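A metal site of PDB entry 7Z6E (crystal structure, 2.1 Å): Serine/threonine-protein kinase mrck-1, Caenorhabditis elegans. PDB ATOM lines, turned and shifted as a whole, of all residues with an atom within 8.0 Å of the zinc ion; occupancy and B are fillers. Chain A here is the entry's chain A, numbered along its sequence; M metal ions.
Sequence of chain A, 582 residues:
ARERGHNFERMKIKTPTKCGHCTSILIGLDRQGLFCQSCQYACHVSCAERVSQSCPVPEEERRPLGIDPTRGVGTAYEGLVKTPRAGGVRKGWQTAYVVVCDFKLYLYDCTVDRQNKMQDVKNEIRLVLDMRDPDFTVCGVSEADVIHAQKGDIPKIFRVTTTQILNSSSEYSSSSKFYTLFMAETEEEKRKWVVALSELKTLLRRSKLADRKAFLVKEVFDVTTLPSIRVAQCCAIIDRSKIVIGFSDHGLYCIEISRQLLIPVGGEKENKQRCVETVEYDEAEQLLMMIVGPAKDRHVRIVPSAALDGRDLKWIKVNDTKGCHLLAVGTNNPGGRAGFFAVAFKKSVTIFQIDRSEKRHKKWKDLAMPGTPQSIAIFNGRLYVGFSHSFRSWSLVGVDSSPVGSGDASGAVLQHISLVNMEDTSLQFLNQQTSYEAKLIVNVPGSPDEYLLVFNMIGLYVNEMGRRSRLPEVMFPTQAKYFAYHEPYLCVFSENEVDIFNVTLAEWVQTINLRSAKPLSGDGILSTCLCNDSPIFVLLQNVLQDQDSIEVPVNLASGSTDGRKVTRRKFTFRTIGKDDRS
The zinc ion is bound by ND1 of His 6 (2.1 Å), SG of Cys 39 (2.3 Å), SG of Cys 36 (2.3 Å) and SG of Cys 55 (2.4 Å).
The side-chain sulfur (SG) of Cys 39 sits close to the backbone NH (N) of Tyr 41 (3.7 Å).
NE2 of His 6 sits at hydrogen-bond distance from O of Ser 52 (3.0 Å).
The backbone NH (N) of Cys 36 lies within hydrogen-bond range of the backbone carbonyl oxygen (O) of Tyr 41 (2.9 Å).
SG of Cys 36 sits close to N of Ser 38, 3.4 Å away.
The side-chain sulfur (SG) of Cys 36 lies close to the backbone NH (N) of Asn 7, 3.5 Å away.
Within 4 Å of the zinc ion: His 6, Cys 36, Cys 39 and Cys 55.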
ATOM      1  N   GLY A   5     -30.430 -20.541 -11.287  1.00  0.00           N
ATOM      2  CA  GLY A   5     -29.398 -19.535 -11.505  1.00  0.00           C
ATOM      3  C   GLY A   5     -28.686 -19.633 -12.842  1.00  0.00           C
ATOM      4  O   GLY A   5     -28.861 -20.611 -13.570  1.00  0.00           O
ATOM      5  N   HIS A   6     -27.876 -18.626 -13.180  1.00  0.00           N
ATOM      6  CA  HIS A   6     -27.235 -18.555 -14.493  1.00  0.00           C
ATOM      7  C   HIS A   6     -26.427 -19.804 -14.814  1.00  0.00           C
ATOM      8  O   HIS A   6     -25.920 -20.496 -13.917  1.00  0.00           O
ATOM      9  CB  HIS A   6     -26.301 -17.350 -14.576  1.00  0.00           C
ATOM     10  CG  HIS A   6     -26.978 -16.035 -14.404  1.00  0.00           C
ATOM     11  ND1 HIS A   6     -27.699 -15.430 -15.405  1.00  0.00           N
ATOM     12  CD2 HIS A   6     -27.026 -15.179 -13.342  1.00  0.00           C
ATOM     13  CE1 HIS A   6     -28.163 -14.269 -14.981  1.00  0.00           C
ATOM     14  NE2 HIS A   6     -27.766 -14.096 -13.733  1.00  0.00           N
ATOM     15  N   ASN A   7     -26.311 -20.092 -16.102  1.00  0.00           N
ATOM     16  CA  ASN A   7     -25.470 -21.171 -16.611  1.00  0.00           C
ATOM     17  C   ASN A   7     -24.349 -20.551 -17.427  1.00  0.00           C
ATOM     18  O   ASN A   7     -24.315 -20.583 -18.667  1.00  0.00           O
ATOM     19  CB  ASN A   7     -26.281 -22.163 -17.429  1.00  0.00           C
ATOM     20  CG  ASN A   7     -27.115 -23.091 -16.579  1.00  0.00           C
ATOM     21  OD1 ASN A   7     -27.780 -22.662 -15.622  1.00  0.00           O
ATOM     22  ND2 ASN A   7     -27.089 -24.381 -16.903  1.00  0.00           N
ATOM     23  N   PHE A   8     -23.401 -19.940 -16.722  1.00  0.00           N
ATOM     24  CA  PHE A   8     -22.320 -19.251 -17.385  1.00  0.00           C
ATOM     25  C   PHE A   8     -21.405 -20.226 -18.099  1.00  0.00           C
ATOM     26  O   PHE A   8     -21.209 -21.370 -17.669  1.00  0.00           O
ATOM     27  CB  PHE A   8     -21.523 -18.429 -16.378  1.00  0.00           C
ATOM     28  CG  PHE A   8     -22.182 -17.136 -16.023  1.00  0.00           C
ATOM     29  CD1 PHE A   8     -22.493 -16.200 -16.992  1.00  0.00           C
ATOM     30  CD2 PHE A   8     -22.512 -16.860 -14.701  1.00  0.00           C
ATOM     31  CE1 PHE A   8     -23.101 -15.013 -16.665  1.00  0.00           C
ATOM     32  CE2 PHE A   8     -23.130 -15.666 -14.363  1.00  0.00           C
ATOM     33  CZ  PHE A   8     -23.420 -14.747 -15.346  1.00  0.00           C
ATOM     34  N   PHE A  35     -20.900 -15.953 -20.642  1.00  0.00           N
ATOM     35  CA  PHE A  35     -22.153 -15.831 -21.373  1.00  0.00           C
ATOM     36  C   PHE A  35     -23.128 -16.854 -20.811  1.00  0.00           C
ATOM     37  O   PHE A  35     -22.739 -18.003 -20.568  1.00  0.00           O
ATOM     38  CB  PHE A  35     -21.931 -16.033 -22.879  1.00  0.00           C
ATOM     39  CG  PHE A  35     -23.210 -16.091 -23.674  1.00  0.00           C
ATOM     40  CD1 PHE A  35     -23.905 -14.926 -23.986  1.00  0.00           C
ATOM     41  CD2 PHE A  35     -23.740 -17.304 -24.077  1.00  0.00           C
ATOM     42  CE1 PHE A  35     -25.109 -14.965 -24.698  1.00  0.00           C
ATOM     43  CE2 PHE A  35     -24.934 -17.363 -24.794  1.00  0.00           C
ATOM     44  CZ  PHE A  35     -25.629 -16.188 -25.103  1.00  0.00           C
ATOM     45  N   CYS A  36     -24.374 -16.438 -20.588  1.00  0.00           N
ATOM     46  CA  CYS A  36     -25.309 -17.288 -19.868  1.00  0.00           C
ATOM     47  C   CYS A  36     -26.094 -18.233 -20.774  1.00  0.00           C
ATOM     48  O   CYS A  36     -26.327 -19.381 -20.386  1.00  0.00           O
ATOM     49  CB  CYS A  36     -26.313 -16.478 -19.052  1.00  0.00           C
ATOM     50  SG  CYS A  36     -27.515 -17.634 -18.264  1.00  0.00           S
ATOM     51  N   GLN A  37     -26.575 -17.771 -21.915  1.00  0.00           N
ATOM     52  CA  GLN A  37     -27.309 -18.660 -22.833  1.00  0.00           C
ATOM     53  C   GLN A  37     -28.727 -18.957 -22.350  1.00  0.00           C
ATOM     54  O   GLN A  37     -29.624 -19.107 -23.167  1.00  0.00           O
ATOM     55  CB  GLN A  37     -26.569 -19.999 -23.060  1.00  0.00           C
ATOM     56  CG  GLN A  37     -27.108 -20.897 -24.186  1.00  0.00           C
ATOM     57  CD  GLN A  37     -26.278 -20.801 -25.468  1.00  0.00           C
ATOM     58  OE1 GLN A  37     -26.642 -20.073 -26.408  1.00  0.00           O
ATOM     59  NE2 GLN A  37     -25.137 -21.494 -25.498  1.00  0.00           N
ATOM     60  N   SER A  38     -28.947 -19.053 -21.036  1.00  0.00           N
ATOM     61  CA  SER A  38     -30.305 -19.129 -20.526  1.00  0.00           C
ATOM     62  C   SER A  38     -31.041 -17.800 -20.657  1.00  0.00           C
ATOM     63  O   SER A  38     -32.247 -17.775 -20.911  1.00  0.00           O
ATOM     64  CB  SER A  38     -30.297 -19.589 -19.062  1.00  0.00           C
ATOM     65  OG  SER A  38     -30.190 -21.003 -18.958  1.00  0.00           O
ATOM     66  N   CYS A  39     -30.324 -16.692 -20.522  1.00  0.00           N
ATOM     67  CA  CYS A  39     -30.904 -15.358 -20.589  1.00  0.00           C
ATOM     68  C   CYS A  39     -30.097 -14.419 -21.479  1.00  0.00           C
ATOM     69  O   CYS A  39     -30.465 -13.246 -21.588  1.00  0.00           O
ATOM     70  CB  CYS A  39     -30.987 -14.752 -19.174  1.00  0.00           C
ATOM     71  SG  CYS A  39     -29.322 -14.567 -18.439  1.00  0.00           S
ATOM     72  N   GLN A  40     -29.005 -14.880 -22.092  1.00  0.00           N
ATOM     73  CA  GLN A  40     -28.185 -14.129 -23.047  1.00  0.00           C
ATOM     74  C   GLN A  40     -27.293 -13.093 -22.378  1.00  0.00           C
ATOM     75  O   GLN A  40     -26.801 -12.188 -23.060  1.00  0.00           O
ATOM     76  CB  GLN A  40     -29.030 -13.422 -24.120  1.00  0.00           C
ATOM     77  CG  GLN A  40     -29.826 -14.350 -25.012  1.00  0.00           C
ATOM     78  CD  GLN A  40     -28.950 -15.067 -26.008  1.00  0.00           C
ATOM     79  OE1 GLN A  40     -27.981 -14.510 -26.508  1.00  0.00           O
ATOM     80  NE2 GLN A  40     -29.297 -16.310 -26.303  1.00  0.00           N
ATOM     81  N   TYR A  41     -27.082 -13.170 -21.070  1.00  0.00           N
ATOM     82  CA  TYR A  41     -26.273 -12.185 -20.369  1.00  0.00           C
ATOM     83  C   TYR A  41     -24.791 -12.425 -20.650  1.00  0.00           C
ATOM     84  O   TYR A  41     -24.319 -13.578 -20.601  1.00  0.00           O
ATOM     85  CB  TYR A  41     -26.575 -12.274 -18.871  1.00  0.00           C
ATOM     86  CG  TYR A  41     -26.118 -11.138 -17.994  1.00  0.00           C
ATOM     87  CD1 TYR A  41     -26.918 -10.020 -17.794  1.00  0.00           C
ATOM     88  CD2 TYR A  41     -24.912 -11.204 -17.313  1.00  0.00           C
ATOM     89  CE1 TYR A  41     -26.499  -8.974 -16.967  1.00  0.00           C
ATOM     90  CE2 TYR A  41     -24.482 -10.167 -16.488  1.00  0.00           C
ATOM     91  CZ  TYR A  41     -25.280  -9.061 -16.323  1.00  0.00           C
ATOM     92  OH  TYR A  41     -24.870  -8.046 -15.495  1.00  0.00           O
ATOM     93  N   ALA A  42     -24.044 -11.356 -20.953  1.00  0.00           N
ATOM     94  CA  ALA A  42     -22.598 -11.434 -21.147  1.00  0.00           C
ATOM     95  C   ALA A  42     -21.898 -10.511 -20.169  1.00  0.00           C
ATOM     96  O   ALA A  42     -22.359  -9.385 -19.944  1.00  0.00           O
ATOM     97  CB  ALA A  42     -22.208 -11.061 -22.577  1.00  0.00           C
ATOM     98  N   VAL A  51     -22.988 -10.169 -10.170  1.00  0.00           N
ATOM     99  CA  VAL A  51     -24.253 -10.170 -10.874  1.00  0.00           C
ATOM    100  C   VAL A  51     -25.305 -10.888 -10.040  1.00  0.00           C
ATOM    101  O   VAL A  51     -25.008 -11.861  -9.334  1.00  0.00           O
ATOM    102  CB  VAL A  51     -24.112 -10.848 -12.254  1.00  0.00           C
ATOM    103  CG1 VAL A  51     -25.368 -10.625 -13.080  1.00  0.00           C
ATOM    104  CG2 VAL A  51     -22.907 -10.304 -12.982  1.00  0.00           C
ATOM    105  N   SER A  52     -26.541 -10.394 -10.117  1.00  0.00           N
ATOM    106  CA  SER A  52     -27.670 -11.068  -9.474  1.00  0.00           C
ATOM    107  C   SER A  52     -27.728 -12.524  -9.916  1.00  0.00           C
ATOM    108  O   SER A  52     -27.450 -12.850 -11.068  1.00  0.00           O
ATOM    109  CB  SER A  52     -28.976 -10.350  -9.824  1.00  0.00           C
ATOM    110  OG  SER A  52     -30.109 -11.109  -9.426  1.00  0.00           O
ATOM    111  N   GLN A  53     -28.087 -13.398  -8.976  1.00  0.00           N
ATOM    112  CA  GLN A  53     -28.123 -14.821  -9.281  1.00  0.00           C
ATOM    113  C   GLN A  53     -29.435 -15.261  -9.909  1.00  0.00           C
ATOM    114  O   GLN A  53     -29.447 -16.223 -10.683  1.00  0.00           O
ATOM    115  CB  GLN A  53     -27.852 -15.644  -8.020  1.00  0.00           C
ATOM    116  CG  GLN A  53     -26.373 -15.961  -7.823  1.00  0.00           C
ATOM    117  CD  GLN A  53     -26.041 -16.351  -6.399  1.00  0.00           C
ATOM    118  OE1 GLN A  53     -26.795 -16.074  -5.462  1.00  0.00           O
ATOM    119  NE2 GLN A  53     -24.903 -16.999  -6.228  1.00  0.00           N
ATOM    120  N   SER A  54     -30.536 -14.580  -9.587  1.00  0.00           N
ATOM    121  CA  SER A  54     -31.781 -14.781 -10.317  1.00  0.00           C
ATOM    122  C   SER A  54     -31.558 -14.542 -11.798  1.00  0.00           C
ATOM    123  O   SER A  54     -31.025 -13.501 -12.197  1.00  0.00           O
ATOM    124  CB  SER A  54     -32.875 -13.851  -9.776  1.00  0.00           C
ATOM    125  OG  SER A  54     -32.760 -13.699  -8.365  1.00  0.00           O
ATOM    126  N   CYS A  55     -31.948 -15.525 -12.626  1.00  0.00           N
ATOM    127  CA  CYS A  55     -31.308 -15.612 -13.933  1.00  0.00           C
ATOM    128  C   CYS A  55     -31.879 -14.558 -14.896  1.00  0.00           C
ATOM    129  O   CYS A  55     -31.138 -13.637 -15.264  1.00  0.00           O
ATOM    130  CB  CYS A  55     -31.418 -17.049 -14.478  1.00  0.00           C
ATOM    131  SG  CYS A  55     -30.834 -17.318 -16.166  1.00  0.00           S
ATOM    132  N   PRO A  56     -33.154 -14.621 -15.317  1.00  0.00           N
ATOM    133  CA  PRO A  56     -33.665 -13.500 -16.110  1.00  0.00           C
ATOM    134  C   PRO A  56     -33.749 -12.256 -15.238  1.00  0.00           C
ATOM    135  O   PRO A  56     -34.755 -12.019 -14.570  1.00  0.00           O
ATOM    136  CB  PRO A  56     -35.071 -13.975 -16.555  1.00  0.00           C
ATOM    137  CG  PRO A  56     -35.109 -15.431 -16.244  1.00  0.00           C
ATOM    138  CD  PRO A  56     -34.187 -15.643 -15.082  1.00  0.00           C
ATOM    139  N   VAL A  57     -32.684 -11.453 -15.221  1.00  0.00           N
ATOM    140  CA  VAL A  57     -32.612 -10.321 -14.278  1.00  0.00           C
ATOM    141  C   VAL A  57     -33.706  -9.310 -14.621  1.00  0.00           C
ATOM    142  O   VAL A  57     -34.025  -9.120 -15.820  1.00  0.00           O
ATOM    143  CB  VAL A  57     -31.222  -9.672 -14.325  1.00  0.00           C
ATOM    144  CG1 VAL A  57     -30.706  -9.431 -12.913  1.00  0.00           C
ATOM    145  CG2 VAL A  57     -30.252 -10.549 -15.089  1.00  0.00           C
HETATM  146 ZN    ZN M   1     -28.870 -16.231 -16.964  1.00  0.00          ZN
